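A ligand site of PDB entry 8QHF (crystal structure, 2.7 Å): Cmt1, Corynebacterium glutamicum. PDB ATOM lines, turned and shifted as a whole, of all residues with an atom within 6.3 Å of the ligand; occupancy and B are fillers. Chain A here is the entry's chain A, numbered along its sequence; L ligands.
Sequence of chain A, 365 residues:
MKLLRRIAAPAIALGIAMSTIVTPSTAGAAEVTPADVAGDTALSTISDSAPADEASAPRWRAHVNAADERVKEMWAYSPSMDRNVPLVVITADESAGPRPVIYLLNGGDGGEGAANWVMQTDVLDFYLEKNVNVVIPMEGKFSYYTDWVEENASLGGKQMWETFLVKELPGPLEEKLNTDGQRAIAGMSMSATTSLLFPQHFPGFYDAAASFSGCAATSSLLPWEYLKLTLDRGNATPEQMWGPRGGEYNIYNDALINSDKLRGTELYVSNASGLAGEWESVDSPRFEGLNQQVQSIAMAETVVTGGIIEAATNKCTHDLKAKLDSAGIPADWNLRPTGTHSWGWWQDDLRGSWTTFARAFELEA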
ATOM      1  N   GLY A 108      19.656 -25.028 -26.126  1.00  0.00           N
ATOM      2  CA  GLY A 108      18.576 -25.755 -26.778  1.00  0.00           C
ATOM      3  C   GLY A 108      18.967 -27.091 -27.371  1.00  0.00           C
ATOM      4  O   GLY A 108      18.179 -28.016 -27.373  1.00  0.00           O
ATOM      5  N   PHE A 142      15.794 -28.709 -25.983  1.00  0.00           N
ATOM      6  CA  PHE A 142      14.580 -27.898 -25.924  1.00  0.00           C
ATOM      7  C   PHE A 142      13.755 -28.115 -24.640  1.00  0.00           C
ATOM      8  O   PHE A 142      12.531 -28.017 -24.669  1.00  0.00           O
ATOM      9  CB  PHE A 142      13.720 -28.103 -27.217  1.00  0.00           C
ATOM     10  CG  PHE A 142      14.551 -28.106 -28.486  1.00  0.00           C
ATOM     11  CD1 PHE A 142      15.309 -27.007 -28.846  1.00  0.00           C
ATOM     12  CD2 PHE A 142      14.695 -29.262 -29.239  1.00  0.00           C
ATOM     13  CE1 PHE A 142      16.137 -27.039 -29.962  1.00  0.00           C
ATOM     14  CE2 PHE A 142      15.535 -29.292 -30.349  1.00  0.00           C
ATOM     15  CZ  PHE A 142      16.248 -28.181 -30.702  1.00  0.00           C
ATOM     16  N   TYR A 144      14.578 -26.593 -21.349  1.00  0.00           N
ATOM     17  CA  TYR A 144      14.806 -25.579 -20.333  1.00  0.00           C
ATOM     18  C   TYR A 144      15.349 -26.176 -19.038  1.00  0.00           C
ATOM     19  O   TYR A 144      15.463 -25.445 -18.051  1.00  0.00           O
ATOM     20  CB  TYR A 144      13.590 -24.667 -20.095  1.00  0.00           C
ATOM     21  CG  TYR A 144      13.561 -23.503 -21.058  1.00  0.00           C
ATOM     22  CD1 TYR A 144      12.980 -23.624 -22.309  1.00  0.00           C
ATOM     23  CD2 TYR A 144      14.172 -22.302 -20.741  1.00  0.00           C
ATOM     24  CE1 TYR A 144      12.982 -22.575 -23.211  1.00  0.00           C
ATOM     25  CE2 TYR A 144      14.204 -21.254 -21.638  1.00  0.00           C
ATOM     26  CZ  TYR A 144      13.612 -21.391 -22.877  1.00  0.00           C
ATOM     27  OH  TYR A 144      13.636 -20.326 -23.748  1.00  0.00           O
ATOM     28  N   MET A 188      23.794 -21.735 -20.778  1.00  0.00           N
ATOM     29  CA  MET A 188      23.822 -20.767 -21.864  1.00  0.00           C
ATOM     30  C   MET A 188      22.517 -20.766 -22.628  1.00  0.00           C
ATOM     31  O   MET A 188      21.877 -21.813 -22.790  1.00  0.00           O
ATOM     32  CB  MET A 188      24.944 -21.085 -22.838  1.00  0.00           C
ATOM     33  CG  MET A 188      24.853 -22.459 -23.388  1.00  0.00           C
ATOM     34  SD  MET A 188      25.769 -22.602 -24.896  1.00  0.00           S
ATOM     35  CE  MET A 188      25.564 -24.333 -25.194  1.00  0.00           C
ATOM     36  N   SER A 189      22.121 -19.593 -23.101  1.00  0.00           N
ATOM     37  CA  SER A 189      20.922 -19.467 -23.900  1.00  0.00           C
ATOM     38  C   SER A 189      19.663 -19.948 -23.150  1.00  0.00           C
ATOM     39  O   SER A 189      19.303 -19.296 -22.172  1.00  0.00           O
ATOM     40  CB  SER A 189      21.112 -20.126 -25.262  1.00  0.00           C
ATOM     41  OG  SER A 189      21.025 -19.121 -26.258  1.00  0.00           O
ATOM     42  N   MET A 190      19.009 -21.063 -23.548  1.00  0.00           N
ATOM     43  CA  MET A 190      17.841 -21.542 -22.819  1.00  0.00           C
ATOM     44  C   MET A 190      18.188 -21.908 -21.360  1.00  0.00           C
ATOM     45  O   MET A 190      17.434 -21.556 -20.456  1.00  0.00           O
ATOM     46  CB  MET A 190      17.149 -22.690 -23.553  1.00  0.00           C
ATOM     47  CG  MET A 190      17.833 -23.998 -23.386  1.00  0.00           C
ATOM     48  SD  MET A 190      16.720 -25.392 -23.443  1.00  0.00           S
ATOM     49  CE  MET A 190      17.779 -26.584 -22.853  1.00  0.00           C
ATOM     50  N   THR A 193      18.481 -19.393 -18.174  1.00  0.00           N
ATOM     51  CA  THR A 193      17.287 -19.180 -17.359  1.00  0.00           C
ATOM     52  C   THR A 193      17.388 -20.214 -16.211  1.00  0.00           C
ATOM     53  O   THR A 193      17.232 -19.868 -15.051  1.00  0.00           O
ATOM     54  CB  THR A 193      15.991 -19.405 -18.190  1.00  0.00           C
ATOM     55  OG1 THR A 193      15.922 -18.448 -19.255  1.00  0.00           O
ATOM     56  CG2 THR A 193      14.731 -19.339 -17.332  1.00  0.00           C
ATOM     57  N   PHE A 212      24.899 -17.431 -19.016  1.00  0.00           N
ATOM     58  CA  PHE A 212      25.543 -16.995 -20.255  1.00  0.00           C
ATOM     59  C   PHE A 212      24.561 -16.663 -21.359  1.00  0.00           C
ATOM     60  O   PHE A 212      24.179 -17.545 -22.127  1.00  0.00           O
ATOM     61  CB  PHE A 212      26.498 -18.085 -20.779  1.00  0.00           C
ATOM     62  CG  PHE A 212      27.535 -18.646 -19.847  1.00  0.00           C
ATOM     63  CD1 PHE A 212      28.178 -17.836 -18.929  1.00  0.00           C
ATOM     64  CD2 PHE A 212      27.919 -19.970 -19.917  1.00  0.00           C
ATOM     65  CE1 PHE A 212      29.157 -18.346 -18.098  1.00  0.00           C
ATOM     66  CE2 PHE A 212      28.904 -20.473 -19.084  1.00  0.00           C
ATOM     67  CZ  PHE A 212      29.516 -19.661 -18.185  1.00  0.00           C
ATOM     68  N   SER A 213      24.171 -15.390 -21.480  1.00  0.00           N
ATOM     69  CA  SER A 213      23.279 -14.890 -22.524  1.00  0.00           C
ATOM     70  C   SER A 213      21.881 -15.532 -22.566  1.00  0.00           C
ATOM     71  O   SER A 213      21.598 -16.312 -23.460  1.00  0.00           O
ATOM     72  CB  SER A 213      23.953 -14.986 -23.884  1.00  0.00           C
ATOM     73  OG  SER A 213      23.486 -13.995 -24.776  1.00  0.00           O
ATOM     74  N   GLY A 214      21.021 -15.142 -21.652  1.00  0.00           N
ATOM     75  CA  GLY A 214      19.658 -15.662 -21.623  1.00  0.00           C
ATOM     76  C   GLY A 214      18.645 -14.627 -21.220  1.00  0.00           C
ATOM     77  O   GLY A 214      18.923 -13.427 -21.249  1.00  0.00           O
ATOM     78  N   CYS A 215      17.452 -15.081 -20.854  1.00  0.00           N
ATOM     79  CA  CYS A 215      16.406 -14.185 -20.381  1.00  0.00           C
ATOM     80  C   CYS A 215      15.877 -14.742 -19.068  1.00  0.00           C
ATOM     81  O   CYS A 215      15.387 -15.866 -19.019  1.00  0.00           O
ATOM     82  CB  CYS A 215      15.299 -14.030 -21.429  1.00  0.00           C
ATOM     83  SG  CYS A 215      14.120 -12.697 -21.076  1.00  0.00           S
ATOM     84  N   TYR A 226       9.637 -15.734 -26.147  1.00  0.00           N
ATOM     85  CA  TYR A 226      10.999 -16.245 -26.356  1.00  0.00           C
ATOM     86  C   TYR A 226      11.095 -17.729 -25.997  1.00  0.00           C
ATOM     87  O   TYR A 226      11.940 -18.442 -26.532  1.00  0.00           O
ATOM     88  CB  TYR A 226      12.015 -15.485 -25.511  1.00  0.00           C
ATOM     89  CG  TYR A 226      11.977 -13.980 -25.567  1.00  0.00           C
ATOM     90  CD1 TYR A 226      11.516 -13.313 -26.697  1.00  0.00           C
ATOM     91  CD2 TYR A 226      12.539 -13.216 -24.557  1.00  0.00           C
ATOM     92  CE1 TYR A 226      11.514 -11.919 -26.764  1.00  0.00           C
ATOM     93  CE2 TYR A 226      12.527 -11.829 -24.603  1.00  0.00           C
ATOM     94  CZ  TYR A 226      12.025 -11.182 -25.711  1.00  0.00           C
ATOM     95  OH  TYR A 226      12.072  -9.808 -25.743  1.00  0.00           O
ATOM     96  N   LEU A 229      10.443 -19.696 -29.144  1.00  0.00           N
ATOM     97  CA  LEU A 229      11.544 -19.862 -30.116  1.00  0.00           C
ATOM     98  C   LEU A 229      12.276 -21.219 -29.891  1.00  0.00           C
ATOM     99  O   LEU A 229      12.563 -21.959 -30.828  1.00  0.00           O
ATOM    100  CB  LEU A 229      12.589 -18.722 -30.002  1.00  0.00           C
ATOM    101  CG  LEU A 229      12.510 -17.530 -30.955  1.00  0.00           C
ATOM    102  CD1 LEU A 229      12.360 -17.963 -32.400  1.00  0.00           C
ATOM    103  CD2 LEU A 229      11.436 -16.578 -30.519  1.00  0.00           C
ATOM    104  N   THR A 230      12.550 -21.527 -28.616  1.00  0.00           N
ATOM    105  CA  THR A 230      13.244 -22.746 -28.259  1.00  0.00           C
ATOM    106  C   THR A 230      12.331 -23.966 -28.328  1.00  0.00           C
ATOM    107  O   THR A 230      12.690 -24.951 -28.952  1.00  0.00           O
ATOM    108  CB  THR A 230      13.873 -22.578 -26.865  1.00  0.00           C
ATOM    109  OG1 THR A 230      14.768 -21.464 -26.888  1.00  0.00           O
ATOM    110  CG2 THR A 230      14.622 -23.815 -26.423  1.00  0.00           C
ATOM    111  N   ARG A 233      11.031 -25.734 -31.761  1.00  0.00           N
ATOM    112  CA  ARG A 233      12.002 -26.657 -32.363  1.00  0.00           C
ATOM    113  C   ARG A 233      11.867 -28.105 -31.845  1.00  0.00           C
ATOM    114  O   ARG A 233      12.315 -29.030 -32.501  1.00  0.00           O
ATOM    115  CB  ARG A 233      13.429 -26.152 -32.169  1.00  0.00           C
ATOM    116  CG  ARG A 233      13.735 -24.821 -32.848  1.00  0.00           C
ATOM    117  CD  ARG A 233      14.347 -24.979 -34.243  1.00  0.00           C
ATOM    118  NE  ARG A 233      15.428 -25.980 -34.306  1.00  0.00           N
ATOM    119  CZ  ARG A 233      16.598 -25.786 -34.902  1.00  0.00           C
ATOM    120  NH1 ARG A 233      16.887 -24.614 -35.458  1.00  0.00           N
ATOM    121  NH2 ARG A 233      17.515 -26.743 -34.905  1.00  0.00           N
ATOM    122  N   GLY A 277      24.360 -17.212 -34.534  1.00  0.00           N
ATOM    123  CA  GLY A 277      24.076 -17.669 -33.180  1.00  0.00           C
ATOM    124  C   GLY A 277      24.439 -19.070 -32.786  1.00  0.00           C
ATOM    125  O   GLY A 277      25.474 -19.603 -33.208  1.00  0.00           O
ATOM    126  N   GLU A 278      23.615 -19.651 -31.921  1.00  0.00           N
ATOM    127  CA  GLU A 278      23.740 -20.964 -31.306  1.00  0.00           C
ATOM    128  C   GLU A 278      23.798 -22.093 -32.336  1.00  0.00           C
ATOM    129  O   GLU A 278      24.474 -23.094 -32.108  1.00  0.00           O
ATOM    130  CB  GLU A 278      22.554 -21.172 -30.364  1.00  0.00           C
ATOM    131  CG  GLU A 278      22.762 -22.248 -29.321  1.00  0.00           C
ATOM    132  CD  GLU A 278      21.627 -22.401 -28.322  1.00  0.00           C
ATOM    133  OE1 GLU A 278      20.548 -21.795 -28.532  1.00  0.00           O
ATOM    134  OE2 GLU A 278      21.826 -23.117 -27.323  1.00  0.00           O
ATOM    135  N   TRP A 279      23.098 -21.924 -33.462  1.00  0.00           N
ATOM    136  CA  TRP A 279      23.023 -22.889 -34.555  1.00  0.00           C
ATOM    137  C   TRP A 279      24.297 -22.956 -35.393  1.00  0.00           C
ATOM    138  O   TRP A 279      24.539 -23.970 -36.047  1.00  0.00           O
ATOM    139  CB  TRP A 279      21.837 -22.520 -35.475  1.00  0.00           C
ATOM    140  CG  TRP A 279      21.880 -21.111 -36.006  1.00  0.00           C
ATOM    141  CD1 TRP A 279      22.533 -20.659 -37.112  1.00  0.00           C
ATOM    142  CD2 TRP A 279      21.240 -19.955 -35.425  1.00  0.00           C
ATOM    143  NE1 TRP A 279      22.401 -19.292 -37.231  1.00  0.00           N
ATOM    144  CE2 TRP A 279      21.591 -18.836 -36.229  1.00  0.00           C
ATOM    145  CE3 TRP A 279      20.435 -19.746 -34.291  1.00  0.00           C
ATOM    146  CZ2 TRP A 279      21.128 -17.546 -35.949  1.00  0.00           C
ATOM    147  CZ3 TRP A 279      20.007 -18.462 -34.001  1.00  0.00           C
ATOM    148  CH2 TRP A 279      20.334 -17.383 -34.839  1.00  0.00           C
ATOM    149  N   ILE A 308      17.795  -9.518 -33.641  1.00  0.00           N
ATOM    150  CA  ILE A 308      16.579  -9.633 -32.823  1.00  0.00           C
ATOM    151  C   ILE A 308      16.896 -10.419 -31.537  1.00  0.00           C
ATOM    152  O   ILE A 308      16.404 -10.075 -30.470  1.00  0.00           O
ATOM    153  CB  ILE A 308      15.414 -10.295 -33.621  1.00  0.00           C
ATOM    154  CG1 ILE A 308      14.947  -9.419 -34.796  1.00  0.00           C
ATOM    155  CG2 ILE A 308      14.256 -10.685 -32.703  1.00  0.00           C
ATOM    156  CD1 ILE A 308      14.057 -10.107 -35.718  1.00  0.00           C
ATOM    157  N   ILE A 309      17.696 -11.478 -31.629  1.00  0.00           N
ATOM    158  CA  ILE A 309      18.055 -12.287 -30.467  1.00  0.00           C
ATOM    159  C   ILE A 309      18.880 -11.467 -29.499  1.00  0.00           C
ATOM    160  O   ILE A 309      18.622 -11.490 -28.293  1.00  0.00           O
ATOM    161  CB  ILE A 309      18.770 -13.592 -30.889  1.00  0.00           C
ATOM    162  CG1 ILE A 309      17.794 -14.551 -31.588  1.00  0.00           C
ATOM    163  CG2 ILE A 309      19.411 -14.277 -29.699  1.00  0.00           C
ATOM    164  CD1 ILE A 309      18.466 -15.683 -32.269  1.00  0.00           C
ATOM    165  N   ALA A 312      16.667  -8.804 -27.692  1.00  0.00           N
ATOM    166  CA  ALA A 312      15.812  -9.479 -26.712  1.00  0.00           C
ATOM    167  C   ALA A 312      16.580  -9.819 -25.423  1.00  0.00           C
ATOM    168  O   ALA A 312      16.079  -9.536 -24.338  1.00  0.00           O
ATOM    169  CB  ALA A 312      15.228 -10.735 -27.332  1.00  0.00           C
ATOM    170  N   THR A 313      17.790 -10.394 -25.537  1.00  0.00           N
ATOM    171  CA  THR A 313      18.651 -10.781 -24.432  1.00  0.00           C
ATOM    172  C   THR A 313      19.209  -9.538 -23.726  1.00  0.00           C
ATOM    173  O   THR A 313      19.342  -9.518 -22.497  1.00  0.00           O
ATOM    174  CB  THR A 313      19.796 -11.619 -25.004  1.00  0.00           C
ATOM    175  OG1 THR A 313      19.260 -12.777 -25.681  1.00  0.00           O
ATOM    176  CG2 THR A 313      20.849 -11.976 -23.983  1.00  0.00           C
ATOM    177  N   CYS A 316      16.522  -8.217 -21.379  1.00  0.00           N
ATOM    178  CA  CYS A 316      16.355  -9.171 -20.292  1.00  0.00           C
ATOM    179  C   CYS A 316      17.445  -9.029 -19.256  1.00  0.00           C
ATOM    180  O   CYS A 316      17.182  -9.100 -18.060  1.00  0.00           O
ATOM    181  CB  CYS A 316      16.312 -10.586 -20.847  1.00  0.00           C
ATOM    182  SG  CYS A 316      14.856 -10.970 -21.854  1.00  0.00           S
ATOM    183  N   TRP A 346      30.654 -17.451 -26.102  1.00  0.00           N
ATOM    184  CA  TRP A 346      30.391 -18.507 -25.127  1.00  0.00           C
ATOM    185  C   TRP A 346      31.655 -19.207 -24.692  1.00  0.00           C
ATOM    186  O   TRP A 346      31.772 -19.526 -23.514  1.00  0.00           O
ATOM    187  CB  TRP A 346      29.323 -19.502 -25.623  1.00  0.00           C
ATOM    188  CG  TRP A 346      27.944 -18.926 -25.509  1.00  0.00           C
ATOM    189  CD1 TRP A 346      27.439 -18.195 -24.473  1.00  0.00           C
ATOM    190  CD2 TRP A 346      26.888 -19.024 -26.481  1.00  0.00           C
ATOM    191  NE1 TRP A 346      26.142 -17.819 -24.745  1.00  0.00           N
ATOM    192  CE2 TRP A 346      25.784 -18.308 -25.973  1.00  0.00           C
ATOM    193  CE3 TRP A 346      26.779 -19.607 -27.750  1.00  0.00           C
ATOM    194  CZ2 TRP A 346      24.583 -18.192 -26.673  1.00  0.00           C
ATOM    195  CZ3 TRP A 346      25.577 -19.533 -28.422  1.00  0.00           C
ATOM    196  CH2 TRP A 346      24.505 -18.806 -27.901  1.00  0.00           C
HETATM  197  C1  LIG L   1      18.601 -18.075 -27.505  1.00  0.00           C
HETATM  198  C2  LIG L   1      18.401 -18.975 -28.791  1.00  0.00           C
HETATM  199  C3  LIG L   1      17.467 -18.309 -29.813  1.00  0.00           C
HETATM  200  C4  LIG L   1      16.449 -19.247 -30.483  1.00  0.00           C
HETATM  201  C5  LIG L   1      17.063 -20.192 -31.534  1.00  0.00           C
HETATM  202  C6  LIG L   1      16.361 -21.558 -31.586  1.00  0.00           C
HETATM  203  C7  LIG L   1      16.819 -22.512 -30.483  1.00  0.00           C
HETATM  204  C8  LIG L   1      17.624 -16.691 -25.568  1.00  0.00           C
HETATM  205  C9  LIG L   1      17.357 -17.831 -26.584  1.00  0.00           C
HETATM  206  C10 LIG L   1      19.826 -18.485 -26.633  1.00  0.00           C
HETATM  207  C11 LIG L   1      15.758 -14.361 -26.802  1.00  0.00           C
HETATM  208  C12 LIG L   1      16.344 -14.503 -25.400  1.00  0.00           C
HETATM  209  C13 LIG L   1      16.379 -15.990 -25.014  1.00  0.00           C
HETATM  210  O1  LIG L   1      19.657 -19.061 -29.450  1.00  0.00           O
HETATM  211  O2  LIG L   1      20.572 -17.275 -26.485  1.00  0.00           O
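The backbone carbonyl oxygen (O) of Ser 213 sits at hydrogen-bond distance from an oxygen (O2) of the ligand (3.3 Å).
OG of Ser 189 is covalently linked to C10 of the ligand.
O1 of the ligand is in hydrogen-bond range of OE1 of Glu 278 (3.0 Å).
The backbone carbonyl oxygen (O) of Ser 213 sits close to the backbone NH (N) of Ser 189 (3.3 Å).
The side-chain sulfur of Cys 215 forms a disulfide with the side-chain sulfur of Cys 316 (2.0 Å).
N of Ser 189 lies within hydrogen-bond range of O of Phe 212 (3.1 Å).
OG1 of Thr 313 sits at hydrogen-bond distance from O of Ile 309 (3.0 Å).
N of Gly 108 is in hydrogen-bond range of OE2 of Glu 278.
Merely in contact with the ligand: Tyr 226 (3.996 Å), Leu 229 (3.9 Å), Ile 309 (3.7 Å), Ala 312 (3.7 Å) and Thr 313 (3.4 Å).
Hydrophobic or aromatic side chains within 4 Å of the ligand: Tyr 226, Leu 229, Ile 309 and Ala 312.
The nearest printed residue that does not touch the ligand is Met 190 (4.1 Å).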
